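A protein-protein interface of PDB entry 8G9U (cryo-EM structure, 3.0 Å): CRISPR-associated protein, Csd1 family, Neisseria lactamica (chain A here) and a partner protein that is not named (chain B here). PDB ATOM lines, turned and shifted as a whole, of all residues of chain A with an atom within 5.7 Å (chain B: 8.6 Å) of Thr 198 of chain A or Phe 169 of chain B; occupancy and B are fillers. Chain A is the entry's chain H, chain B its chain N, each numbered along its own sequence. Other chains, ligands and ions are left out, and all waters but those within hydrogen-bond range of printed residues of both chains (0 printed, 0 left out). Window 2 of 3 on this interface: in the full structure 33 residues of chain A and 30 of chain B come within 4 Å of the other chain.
The side-chain sulfur (SG) of Cys 195 of chain A is in hydrogen-bond range of the side-chain hydroxyl (OG1) of Thr 198 of chain A (3.2 Å). The backbone carbonyl oxygen of Lys 200 of chain A lies within hydrogen-bond range of the backbone NH of Cys 195 of chain A, at 2.8 Å. NZ of Lys 200 of chain A lies within hydrogen-bond range of O of Thr 198 of chain A (3.0 Å). OE2 of Glu 17 of chain B lies within salt-bridge range of NH2 of Arg 15 of chain B. NH1 of Arg 15 of chain B sits at hydrogen-bond distance from O of Phe 167 of chain B (3.3 Å). The side-chain hydroxyl (OH) of Tyr 25 of chain B lies within hydrogen-bond range of the backbone NH (N) of Leu 171 of chain B (3.1 Å).
Printed residues of chain A that touch a printed residue of chain B: Met 1, Cys 195, Leu 196, Val 197, Thr 198 and Gly 199. Hydrophobic or aromatic side chains of chain A within 4 Å of the printed part of chain B: Met 1 and Leu 196. Of the 20 printed residues of chain B, 8 touch a printed residue of chain A. Printed residues of chain B that touch a printed residue of chain A: Arg 15, Ser 16, Glu 17, Tyr 25, Pro 26, Phe 167, Phe 169 and Met 190. Hydrophobic or aromatic side chains of chain B that line the printed part of chain A: Tyr 25, Pro 26, Phe 169 and Met 190. Among the printed residues, no Asp or Glu carboxylate lies within 4 Å of a Lys or Arg side-chain nitrogen of the other chain.
Printed residues of chain B within 4 Å of Cys 195 of chain A: Met 190. Printed residues of chain B within 4 Å of Leu 196 of chain A: Ser 16 (3.5 Å), Glu 17 (3.1 Å), Tyr 25 (3.7 Å), Phe 169 (3.3 Å) and Met 190 (3.3 Å). Val 197 of chain A touches just one residue of chain B: Phe 169 (3.9 Å). Of chain B, only Phe 169 comes within 4 Å of Thr 198 of chain A. Ala 246 of chain A touches none of the printed residues of chain B. Of the printed residues of chain A, Arg 15 of chain B touches Met 1 (2.8 Å). Of the printed residues of chain A, Tyr 25 of chain B touches Leu 196. Phe 169 of chain B touches four residues of chain A. Of the printed residues of chain A, Met 190 of chain B touches Cys 195 (3.5 Å) and Leu 196 (3.3 Å). The nearest residue of chain B that does not touch Thr 198 of chain A is Tyr 192 of chain B (5.1 Å).
The backbone NH (N) of Met 1 of chain A lies close to the guanidinium group (NH1) of Arg 15 of chain B (2.8 Å). The side-chain sulfur of Met 190 of chain B lies close to the backbone carbonyl oxygen of Cys 195 of chain A (3.5 Å).
Among the printed residues, merely in contact across the chains: Thr 198 of chain A with Phe 169 of chain B, Leu 196 of chain A with Glu 17 of chain B, Leu 196 of chain A with Phe 169 of chain B, Leu 196 of chain A with Met 190 of chain B, Met 1 of chain A with Pro 26 of chain B, Leu 196 of chain A with Ser 16 of chain B, Leu 196 of chain A with Tyr 25 of chain B, Met 1 of chain A with Phe 167 of chain B, Gly 199 of chain A with Phe 169 of chain B and Val 197 of chain A with Phe 169 of chain B.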
ATOM      1  N   MET A   1      -8.291 -20.721 -26.002  1.00  0.00           N
ATOM      2  CA  MET A   1      -8.423 -20.742 -24.559  1.00  0.00           C
ATOM      3  C   MET A   1      -9.811 -21.207 -24.191  1.00  0.00           C
ATOM      4  O   MET A   1     -10.065 -21.523 -23.044  1.00  0.00           O
ATOM      5  CB  MET A   1      -8.187 -19.366 -23.959  1.00  0.00           C
ATOM      6  CG  MET A   1      -9.247 -18.375 -24.364  1.00  0.00           C
ATOM      7  SD  MET A   1      -8.961 -16.731 -23.704  1.00  0.00           S
ATOM      8  CE  MET A   1     -10.369 -15.866 -24.382  1.00  0.00           C
ATOM      9  N   HIS A   4      -8.607 -25.085 -24.592  1.00  0.00           N
ATOM     10  CA  HIS A   4      -7.473 -25.424 -23.755  1.00  0.00           C
ATOM     11  C   HIS A   4      -7.745 -25.138 -22.299  1.00  0.00           C
ATOM     12  O   HIS A   4      -7.000 -25.616 -21.449  1.00  0.00           O
ATOM     13  CB  HIS A   4      -6.210 -24.688 -24.175  1.00  0.00           C
ATOM     14  CG  HIS A   4      -4.986 -25.185 -23.477  1.00  0.00           C
ATOM     15  ND1 HIS A   4      -4.295 -24.425 -22.562  1.00  0.00           N
ATOM     16  CD2 HIS A   4      -4.367 -26.387 -23.513  1.00  0.00           C
ATOM     17  CE1 HIS A   4      -3.279 -25.124 -22.090  1.00  0.00           C
ATOM     18  NE2 HIS A   4      -3.302 -26.320 -22.651  1.00  0.00           N
ATOM     19  N   THR A   7      -9.657 -28.651 -21.904  1.00  0.00           N
ATOM     20  CA  THR A   7      -8.654 -29.700 -21.835  1.00  0.00           C
ATOM     21  C   THR A   7      -7.888 -29.604 -20.532  1.00  0.00           C
ATOM     22  O   THR A   7      -7.620 -30.621 -19.878  1.00  0.00           O
ATOM     23  CB  THR A   7      -7.703 -29.597 -23.025  1.00  0.00           C
ATOM     24  OG1 THR A   7      -8.354 -30.078 -24.206  1.00  0.00           O
ATOM     25  CG2 THR A   7      -6.439 -30.393 -22.780  1.00  0.00           C
ATOM     26  N   GLN A  11      -7.638 -32.611 -17.675  1.00  0.00           N
ATOM     27  CA  GLN A  11      -6.378 -33.070 -17.117  1.00  0.00           C
ATOM     28  C   GLN A  11      -6.246 -32.754 -15.637  1.00  0.00           C
ATOM     29  O   GLN A  11      -5.310 -33.246 -15.002  1.00  0.00           O
ATOM     30  CB  GLN A  11      -5.220 -32.455 -17.891  1.00  0.00           C
ATOM     31  CG  GLN A  11      -4.966 -33.149 -19.199  1.00  0.00           C
ATOM     32  CD  GLN A  11      -4.617 -32.182 -20.292  1.00  0.00           C
ATOM     33  OE1 GLN A  11      -4.767 -30.973 -20.130  1.00  0.00           O
ATOM     34  NE2 GLN A  11      -4.154 -32.704 -21.421  1.00  0.00           N
ATOM     35  N   CYS A 195      -2.466 -30.314 -33.118  1.00  0.00           N
ATOM     36  CA  CYS A 195      -3.539 -29.907 -32.215  1.00  0.00           C
ATOM     37  C   CYS A 195      -3.790 -28.410 -32.228  1.00  0.00           C
ATOM     38  O   CYS A 195      -2.867 -27.599 -32.151  1.00  0.00           O
ATOM     39  CB  CYS A 195      -3.244 -30.323 -30.780  1.00  0.00           C
ATOM     40  SG  CYS A 195      -3.641 -31.994 -30.379  1.00  0.00           S
ATOM     41  N   LEU A 196      -5.066 -28.056 -32.302  1.00  0.00           N
ATOM     42  CA  LEU A 196      -5.493 -26.706 -31.972  1.00  0.00           C
ATOM     43  C   LEU A 196      -5.342 -26.423 -30.492  1.00  0.00           C
ATOM     44  O   LEU A 196      -4.891 -25.342 -30.103  1.00  0.00           O
ATOM     45  CB  LEU A 196      -6.941 -26.526 -32.383  1.00  0.00           C
ATOM     46  CG  LEU A 196      -7.564 -25.148 -32.421  1.00  0.00           C
ATOM     47  CD1 LEU A 196      -7.220 -24.383 -33.648  1.00  0.00           C
ATOM     48  CD2 LEU A 196      -9.023 -25.401 -32.375  1.00  0.00           C
ATOM     49  N   VAL A 197      -5.717 -27.379 -29.652  1.00  0.00           N
ATOM     50  CA  VAL A 197      -5.837 -27.115 -28.225  1.00  0.00           C
ATOM     51  C   VAL A 197      -4.484 -27.224 -27.546  1.00  0.00           C
ATOM     52  O   VAL A 197      -3.994 -26.265 -26.941  1.00  0.00           O
ATOM     53  CB  VAL A 197      -6.855 -28.075 -27.593  1.00  0.00           C
ATOM     54  CG1 VAL A 197      -6.744 -28.028 -26.104  1.00  0.00           C
ATOM     55  CG2 VAL A 197      -8.249 -27.705 -28.021  1.00  0.00           C
ATOM     56  N   THR A 198      -3.861 -28.392 -27.643  1.00  0.00           N
ATOM     57  CA  THR A 198      -2.601 -28.614 -26.957  1.00  0.00           C
ATOM     58  C   THR A 198      -1.407 -28.171 -27.785  1.00  0.00           C
ATOM     59  O   THR A 198      -0.364 -27.830 -27.221  1.00  0.00           O
ATOM     60  CB  THR A 198      -2.461 -30.090 -26.597  1.00  0.00           C
ATOM     61  OG1 THR A 198      -2.222 -30.851 -27.786  1.00  0.00           O
ATOM     62  CG2 THR A 198      -3.729 -30.589 -25.938  1.00  0.00           C
ATOM     63  N   GLY A 199      -1.530 -28.169 -29.107  1.00  0.00           N
ATOM     64  CA  GLY A 199      -0.415 -27.862 -29.971  1.00  0.00           C
ATOM     65  C   GLY A 199       0.485 -29.032 -30.284  1.00  0.00           C
ATOM     66  O   GLY A 199       1.419 -28.878 -31.077  1.00  0.00           O
ATOM     67  N   LYS A 200       0.232 -30.197 -29.701  1.00  0.00           N
ATOM     68  CA  LYS A 200       1.054 -31.372 -29.936  1.00  0.00           C
ATOM     69  C   LYS A 200       0.663 -32.028 -31.256  1.00  0.00           C
ATOM     70  O   LYS A 200      -0.301 -31.633 -31.911  1.00  0.00           O
ATOM     71  CB  LYS A 200       0.915 -32.350 -28.775  1.00  0.00           C
ATOM     72  CG  LYS A 200       1.100 -31.708 -27.418  1.00  0.00           C
ATOM     73  CD  LYS A 200       2.494 -31.133 -27.280  1.00  0.00           C
ATOM     74  CE  LYS A 200       2.693 -30.492 -25.920  1.00  0.00           C
ATOM     75  NZ  LYS A 200       1.904 -29.239 -25.785  1.00  0.00           N
ATOM     76  N   ALA A 202      -0.408 -35.399 -31.933  1.00  0.00           N
ATOM     77  CA  ALA A 202      -1.698 -35.843 -31.418  1.00  0.00           C
ATOM     78  C   ALA A 202      -2.765 -35.942 -32.500  1.00  0.00           C
ATOM     79  O   ALA A 202      -3.532 -34.993 -32.690  1.00  0.00           O
ATOM     80  CB  ALA A 202      -2.160 -34.929 -30.290  1.00  0.00           C
ATOM     81  N   GLN A 245      -6.898 -36.960 -28.588  1.00  0.00           N
ATOM     82  CA  GLN A 245      -6.704 -36.919 -27.148  1.00  0.00           C
ATOM     83  C   GLN A 245      -7.110 -35.585 -26.552  1.00  0.00           C
ATOM     84  O   GLN A 245      -7.395 -35.526 -25.359  1.00  0.00           O
ATOM     85  CB  GLN A 245      -5.249 -37.220 -26.802  1.00  0.00           C
ATOM     86  CG  GLN A 245      -5.061 -37.822 -25.426  1.00  0.00           C
ATOM     87  CD  GLN A 245      -4.760 -36.780 -24.375  1.00  0.00           C
ATOM     88  OE1 GLN A 245      -4.167 -35.743 -24.666  1.00  0.00           O
ATOM     89  NE2 GLN A 245      -5.167 -37.048 -23.144  1.00  0.00           N
ATOM     90  N   ALA A 246      -7.129 -34.517 -27.339  1.00  0.00           N
ATOM     91  CA  ALA A 246      -7.594 -33.228 -26.851  1.00  0.00           C
ATOM     92  C   ALA A 246      -9.057 -32.981 -27.154  1.00  0.00           C
ATOM     93  O   ALA A 246      -9.741 -32.333 -26.362  1.00  0.00           O
ATOM     94  CB  ALA A 246      -6.766 -32.094 -27.455  1.00  0.00           C
ATOM     95  N   GLU A 249     -10.899 -34.815 -24.583  1.00  0.00           N
ATOM     96  CA  GLU A 249     -10.785 -34.224 -23.261  1.00  0.00           C
ATOM     97  C   GLU A 249     -11.756 -33.074 -23.087  1.00  0.00           C
ATOM     98  O   GLU A 249     -12.484 -33.028 -22.096  1.00  0.00           O
ATOM     99  CB  GLU A 249      -9.354 -33.786 -22.994  1.00  0.00           C
ATOM    100  CG  GLU A 249      -8.474 -34.968 -22.707  1.00  0.00           C
ATOM    101  CD  GLU A 249      -7.088 -34.585 -22.287  1.00  0.00           C
ATOM    102  OE1 GLU A 249      -6.777 -33.384 -22.307  1.00  0.00           O
ATOM    103  OE2 GLU A 249      -6.301 -35.488 -21.943  1.00  0.00           O
ATOM    104  N   ARG B  15     -11.778 -18.173 -33.929  1.00  0.00           N
ATOM    105  CA  ARG B  15     -11.075 -19.373 -33.523  1.00  0.00           C
ATOM    106  C   ARG B  15     -11.441 -20.494 -34.470  1.00  0.00           C
ATOM    107  O   ARG B  15     -12.609 -20.657 -34.827  1.00  0.00           O
ATOM    108  CB  ARG B  15     -11.461 -19.749 -32.095  1.00  0.00           C
ATOM    109  CG  ARG B  15     -11.030 -18.759 -31.055  1.00  0.00           C
ATOM    110  CD  ARG B  15     -11.017 -19.356 -29.670  1.00  0.00           C
ATOM    111  NE  ARG B  15      -9.891 -18.827 -28.924  1.00  0.00           N
ATOM    112  CZ  ARG B  15      -8.740 -19.463 -28.778  1.00  0.00           C
ATOM    113  NH1 ARG B  15      -7.754 -18.899 -28.096  1.00  0.00           N
ATOM    114  NH2 ARG B  15      -8.573 -20.663 -29.312  1.00  0.00           N
ATOM    115  N   SER B  16     -10.441 -21.252 -34.906  1.00  0.00           N
ATOM    116  CA  SER B  16     -10.740 -22.390 -35.756  1.00  0.00           C
ATOM    117  C   SER B  16     -11.769 -23.293 -35.100  1.00  0.00           C
ATOM    118  O   SER B  16     -12.701 -23.761 -35.759  1.00  0.00           O
ATOM    119  CB  SER B  16      -9.464 -23.162 -36.074  1.00  0.00           C
ATOM    120  OG  SER B  16      -8.586 -22.385 -36.868  1.00  0.00           O
ATOM    121  N   GLU B  17     -11.635 -23.525 -33.792  1.00  0.00           N
ATOM    122  CA  GLU B  17     -12.568 -24.406 -33.096  1.00  0.00           C
ATOM    123  C   GLU B  17     -13.991 -23.881 -33.184  1.00  0.00           C
ATOM    124  O   GLU B  17     -14.910 -24.599 -33.587  1.00  0.00           O
ATOM    125  CB  GLU B  17     -12.149 -24.575 -31.636  1.00  0.00           C
ATOM    126  CG  GLU B  17     -12.033 -23.297 -30.815  1.00  0.00           C
ATOM    127  CD  GLU B  17     -10.609 -22.828 -30.628  1.00  0.00           C
ATOM    128  OE1 GLU B  17      -9.938 -22.543 -31.638  1.00  0.00           O
ATOM    129  OE2 GLU B  17     -10.160 -22.735 -29.467  1.00  0.00           O
ATOM    130  N   TYR B  25     -10.617 -15.115 -31.825  1.00  0.00           N
ATOM    131  CA  TYR B  25      -9.385 -15.235 -31.074  1.00  0.00           C
ATOM    132  C   TYR B  25      -9.239 -13.968 -30.251  1.00  0.00           C
ATOM    133  O   TYR B  25      -9.531 -12.879 -30.754  1.00  0.00           O
ATOM    134  CB  TYR B  25      -8.188 -15.400 -31.998  1.00  0.00           C
ATOM    135  CG  TYR B  25      -7.917 -16.816 -32.401  1.00  0.00           C
ATOM    136  CD1 TYR B  25      -7.746 -17.798 -31.453  1.00  0.00           C
ATOM    137  CD2 TYR B  25      -7.828 -17.168 -33.727  1.00  0.00           C
ATOM    138  CE1 TYR B  25      -7.498 -19.094 -31.816  1.00  0.00           C
ATOM    139  CE2 TYR B  25      -7.579 -18.458 -34.098  1.00  0.00           C
ATOM    140  CZ  TYR B  25      -7.417 -19.419 -33.137  1.00  0.00           C
ATOM    141  OH  TYR B  25      -7.169 -20.717 -33.498  1.00  0.00           O
ATOM    142  N   PRO B  26      -8.819 -14.056 -28.996  1.00  0.00           N
ATOM    143  CA  PRO B  26      -8.876 -12.873 -28.134  1.00  0.00           C
ATOM    144  C   PRO B  26      -8.094 -11.705 -28.676  1.00  0.00           C
ATOM    145  O   PRO B  26      -8.427 -10.558 -28.368  1.00  0.00           O
ATOM    146  CB  PRO B  26      -8.287 -13.374 -26.815  1.00  0.00           C
ATOM    147  CG  PRO B  26      -8.360 -14.843 -26.906  1.00  0.00           C
ATOM    148  CD  PRO B  26      -8.179 -15.189 -28.325  1.00  0.00           C
ATOM    149  N   PRO B  30      -2.023 -13.870 -35.980  1.00  0.00           N
ATOM    150  CA  PRO B  30      -0.894 -13.517 -36.848  1.00  0.00           C
ATOM    151  C   PRO B  30      -1.133 -13.835 -38.299  1.00  0.00           C
ATOM    152  O   PRO B  30      -0.388 -13.337 -39.145  1.00  0.00           O
ATOM    153  CB  PRO B  30       0.257 -14.349 -36.283  1.00  0.00           C
ATOM    154  CG  PRO B  30      -0.111 -14.561 -34.892  1.00  0.00           C
ATOM    155  CD  PRO B  30      -1.596 -14.722 -34.866  1.00  0.00           C
ATOM    156  N   ASP B 166      -2.277 -15.502 -21.244  1.00  0.00           N
ATOM    157  CA  ASP B 166      -1.742 -16.343 -22.307  1.00  0.00           C
ATOM    158  C   ASP B 166      -2.922 -16.977 -23.024  1.00  0.00           C
ATOM    159  O   ASP B 166      -3.620 -17.821 -22.457  1.00  0.00           O
ATOM    160  CB  ASP B 166      -0.813 -17.409 -21.739  1.00  0.00           C
ATOM    161  CG  ASP B 166      -0.412 -18.436 -22.769  1.00  0.00           C
ATOM    162  OD1 ASP B 166       0.562 -18.189 -23.508  1.00  0.00           O
ATOM    163  OD2 ASP B 166      -1.072 -19.491 -22.844  1.00  0.00           O
ATOM    164  N   PHE B 167      -3.147 -16.576 -24.261  1.00  0.00           N
ATOM    165  CA  PHE B 167      -4.336 -17.039 -24.959  1.00  0.00           C
ATOM    166  C   PHE B 167      -4.191 -18.416 -25.498  1.00  0.00           C
ATOM    167  O   PHE B 167      -5.040 -18.876 -26.266  1.00  0.00           O
ATOM    168  CB  PHE B 167      -4.679 -16.058 -26.074  1.00  0.00           C
ATOM    169  CG  PHE B 167      -4.669 -14.636 -25.630  1.00  0.00           C
ATOM    170  CD1 PHE B 167      -5.665 -14.149 -24.818  1.00  0.00           C
ATOM    171  CD2 PHE B 167      -3.660 -13.786 -26.016  1.00  0.00           C
ATOM    172  CE1 PHE B 167      -5.653 -12.845 -24.406  1.00  0.00           C
ATOM    173  CE2 PHE B 167      -3.643 -12.485 -25.605  1.00  0.00           C
ATOM    174  CZ  PHE B 167      -4.639 -12.012 -24.801  1.00  0.00           C
ATOM    175  N   GLY B 168      -3.130 -19.104 -25.106  1.00  0.00           N
ATOM    176  CA  GLY B 168      -2.977 -20.469 -25.519  1.00  0.00           C
ATOM    177  C   GLY B 168      -2.596 -20.551 -26.980  1.00  0.00           C
ATOM    178  O   GLY B 168      -2.065 -19.614 -27.574  1.00  0.00           O
ATOM    179  N   PHE B 169      -2.886 -21.704 -27.563  1.00  0.00           N
ATOM    180  CA  PHE B 169      -2.476 -21.979 -28.932  1.00  0.00           C
ATOM    181  C   PHE B 169      -3.457 -21.317 -29.878  1.00  0.00           C
ATOM    182  O   PHE B 169      -4.577 -21.789 -30.073  1.00  0.00           O
ATOM    183  CB  PHE B 169      -2.380 -23.474 -29.173  1.00  0.00           C
ATOM    184  CG  PHE B 169      -1.010 -24.004 -28.975  1.00  0.00           C
ATOM    185  CD1 PHE B 169      -0.095 -23.975 -29.997  1.00  0.00           C
ATOM    186  CD2 PHE B 169      -0.623 -24.492 -27.755  1.00  0.00           C
ATOM    187  CE1 PHE B 169       1.175 -24.446 -29.815  1.00  0.00           C
ATOM    188  CE2 PHE B 169       0.640 -24.965 -27.568  1.00  0.00           C
ATOM    189  CZ  PHE B 169       1.544 -24.941 -28.598  1.00  0.00           C
ATOM    190  N   MET B 170      -3.030 -20.208 -30.460  1.00  0.00           N
ATOM    191  CA  MET B 170      -3.797 -19.526 -31.481  1.00  0.00           C
ATOM    192  C   MET B 170      -3.297 -19.939 -32.850  1.00  0.00           C
ATOM    193  O   MET B 170      -2.131 -20.303 -33.018  1.00  0.00           O
ATOM    194  CB  MET B 170      -3.663 -18.018 -31.343  1.00  0.00           C
ATOM    195  CG  MET B 170      -4.331 -17.431 -30.145  1.00  0.00           C
ATOM    196  SD  MET B 170      -5.071 -15.891 -30.647  1.00  0.00           S
ATOM    197  CE  MET B 170      -3.615 -15.081 -31.277  1.00  0.00           C
ATOM    198  N   LEU B 171      -4.189 -19.879 -33.832  1.00  0.00           N
ATOM    199  CA  LEU B 171      -3.775 -20.059 -35.212  1.00  0.00           C
ATOM    200  C   LEU B 171      -2.720 -19.024 -35.552  1.00  0.00           C
ATOM    201  O   LEU B 171      -2.937 -17.828 -35.375  1.00  0.00           O
ATOM    202  CB  LEU B 171      -4.973 -19.921 -36.140  1.00  0.00           C
ATOM    203  CG  LEU B 171      -4.664 -19.856 -37.627  1.00  0.00           C
ATOM    204  CD1 LEU B 171      -4.012 -21.138 -38.071  1.00  0.00           C
ATOM    205  CD2 LEU B 171      -5.941 -19.627 -38.386  1.00  0.00           C
ATOM    206  N   TYR B 172      -1.553 -19.482 -35.992  1.00  0.00           N
ATOM    207  CA  TYR B 172      -0.486 -18.533 -36.293  1.00  0.00           C
ATOM    208  C   TYR B 172      -0.653 -17.956 -37.691  1.00  0.00           C
ATOM    209  O   TYR B 172      -0.932 -16.767 -37.857  1.00  0.00           O
ATOM    210  CB  TYR B 172       0.876 -19.212 -36.145  1.00  0.00           C
ATOM    211  CG  TYR B 172       2.000 -18.414 -36.736  1.00  0.00           C
ATOM    212  CD1 TYR B 172       2.432 -17.245 -36.140  1.00  0.00           C
ATOM    213  CD2 TYR B 172       2.627 -18.828 -37.895  1.00  0.00           C
ATOM    214  CE1 TYR B 172       3.452 -16.511 -36.684  1.00  0.00           C
ATOM    215  CE2 TYR B 172       3.648 -18.100 -38.446  1.00  0.00           C
ATOM    216  CZ  TYR B 172       4.058 -16.944 -37.836  1.00  0.00           C
ATOM    217  OH  TYR B 172       5.082 -16.217 -38.389  1.00  0.00           O
ATOM    218  N   GLU B 188      -2.555 -25.714 -40.917  1.00  0.00           N
ATOM    219  CA  GLU B 188      -2.586 -24.662 -39.915  1.00  0.00           C
ATOM    220  C   GLU B 188      -1.393 -24.810 -38.990  1.00  0.00           C
ATOM    221  O   GLU B 188      -1.331 -25.795 -38.243  1.00  0.00           O
ATOM    222  CB  GLU B 188      -3.872 -24.742 -39.110  1.00  0.00           C
ATOM    223  CG  GLU B 188      -5.124 -24.377 -39.835  1.00  0.00           C
ATOM    224  CD  GLU B 188      -5.764 -25.567 -40.497  1.00  0.00           C
ATOM    225  OE1 GLU B 188      -5.111 -26.627 -40.552  1.00  0.00           O
ATOM    226  OE2 GLU B 188      -6.922 -25.452 -40.948  1.00  0.00           O
ATOM    227  N   PRO B 189      -0.428 -23.900 -38.995  1.00  0.00           N
ATOM    228  CA  PRO B 189       0.512 -23.847 -37.879  1.00  0.00           C
ATOM    229  C   PRO B 189      -0.015 -22.919 -36.803  1.00  0.00           C
ATOM    230  O   PRO B 189      -0.671 -21.913 -37.071  1.00  0.00           O
ATOM    231  CB  PRO B 189       1.796 -23.302 -38.521  1.00  0.00           C
ATOM    232  CG  PRO B 189       1.345 -22.531 -39.629  1.00  0.00           C
ATOM    233  CD  PRO B 189       0.126 -23.223 -40.173  1.00  0.00           C
ATOM    234  N   MET B 190       0.255 -23.298 -35.561  1.00  0.00           N
ATOM    235  CA  MET B 190      -0.352 -22.658 -34.411  1.00  0.00           C
ATOM    236  C   MET B 190       0.739 -22.389 -33.394  1.00  0.00           C
ATOM    237  O   MET B 190       1.796 -23.020 -33.415  1.00  0.00           O
ATOM    238  CB  MET B 190      -1.443 -23.543 -33.821  1.00  0.00           C
ATOM    239  CG  MET B 190      -2.385 -23.999 -34.886  1.00  0.00           C
ATOM    240  SD  MET B 190      -3.731 -25.015 -34.350  1.00  0.00           S
ATOM    241  CE  MET B 190      -4.726 -24.917 -35.817  1.00  0.00           C
ATOM    242  N   PHE B 191       0.483 -21.442 -32.501  1.00  0.00           N
ATOM    243  CA  PHE B 191       1.541 -21.017 -31.605  1.00  0.00           C
ATOM    244  C   PHE B 191       0.950 -20.700 -30.243  1.00  0.00           C
ATOM    245  O   PHE B 191      -0.132 -20.115 -30.156  1.00  0.00           O
ATOM    246  CB  PHE B 191       2.283 -19.807 -32.197  1.00  0.00           C
ATOM    247  CG  PHE B 191       1.545 -18.502 -32.078  1.00  0.00           C
ATOM    248  CD1 PHE B 191       0.323 -18.320 -32.679  1.00  0.00           C
ATOM    249  CD2 PHE B 191       2.137 -17.417 -31.472  1.00  0.00           C
ATOM    250  CE1 PHE B 191      -0.337 -17.116 -32.580  1.00  0.00           C
ATOM    251  CE2 PHE B 191       1.484 -16.214 -31.386  1.00  0.00           C
ATOM    252  CZ  PHE B 191       0.250 -16.064 -31.937  1.00  0.00           C
ATOM    253  N   TYR B 192       1.632 -21.146 -29.186  1.00  0.00           N
ATOM    254  CA  TYR B 192       1.491 -20.476 -27.905  1.00  0.00           C
ATOM    255  C   TYR B 192       1.658 -19.004 -28.171  1.00  0.00           C
ATOM    256  O   TYR B 192       2.562 -18.620 -28.913  1.00  0.00           O
ATOM    257  CB  TYR B 192       2.556 -20.929 -26.908  1.00  0.00           C
ATOM    258  CG  TYR B 192       2.149 -22.014 -25.953  1.00  0.00           C
ATOM    259  CD1 TYR B 192       1.076 -21.841 -25.099  1.00  0.00           C
ATOM    260  CD2 TYR B 192       2.886 -23.184 -25.853  1.00  0.00           C
ATOM    261  CE1 TYR B 192       0.710 -22.828 -24.205  1.00  0.00           C
ATOM    262  CE2 TYR B 192       2.535 -24.175 -24.961  1.00  0.00           C
ATOM    263  CZ  TYR B 192       1.446 -23.993 -24.138  1.00  0.00           C
ATOM    264  OH  TYR B 192       1.091 -24.980 -23.248  1.00  0.00           O
ATOM    265  N   GLN B 193       0.776 -18.188 -27.597  1.00  0.00           N
ATOM    266  CA  GLN B 193       0.803 -16.759 -27.866  1.00  0.00           C
ATOM    267  C   GLN B 193       2.250 -16.288 -27.795  1.00  0.00           C
ATOM    268  O   GLN B 193       2.884 -16.018 -28.819  1.00  0.00           O
ATOM    269  CB  GLN B 193      -0.062 -16.065 -26.821  1.00  0.00           C
ATOM    270  CG  GLN B 193      -0.583 -14.737 -27.205  1.00  0.00           C
ATOM    271  CD  GLN B 193      -1.491 -14.822 -28.383  1.00  0.00           C
ATOM    272  OE1 GLN B 193      -1.375 -14.047 -29.330  1.00  0.00           O
ATOM    273  NE2 GLN B 193      -2.393 -15.784 -28.350  1.00  0.00           N
ATOM    274  N   CYS B 194       2.768 -16.152 -26.588  1.00  0.00           N
ATOM    275  CA  CYS B 194       3.800 -16.980 -25.982  1.00  0.00           C
ATOM    276  C   CYS B 194       3.264 -16.885 -24.573  1.00  0.00           C
ATOM    277  O   CYS B 194       3.372 -17.773 -23.721  1.00  0.00           O
ATOM    278  CB  CYS B 194       5.209 -16.418 -26.155  1.00  0.00           C
ATOM    279  SG  CYS B 194       6.509 -17.468 -25.475  1.00  0.00           S
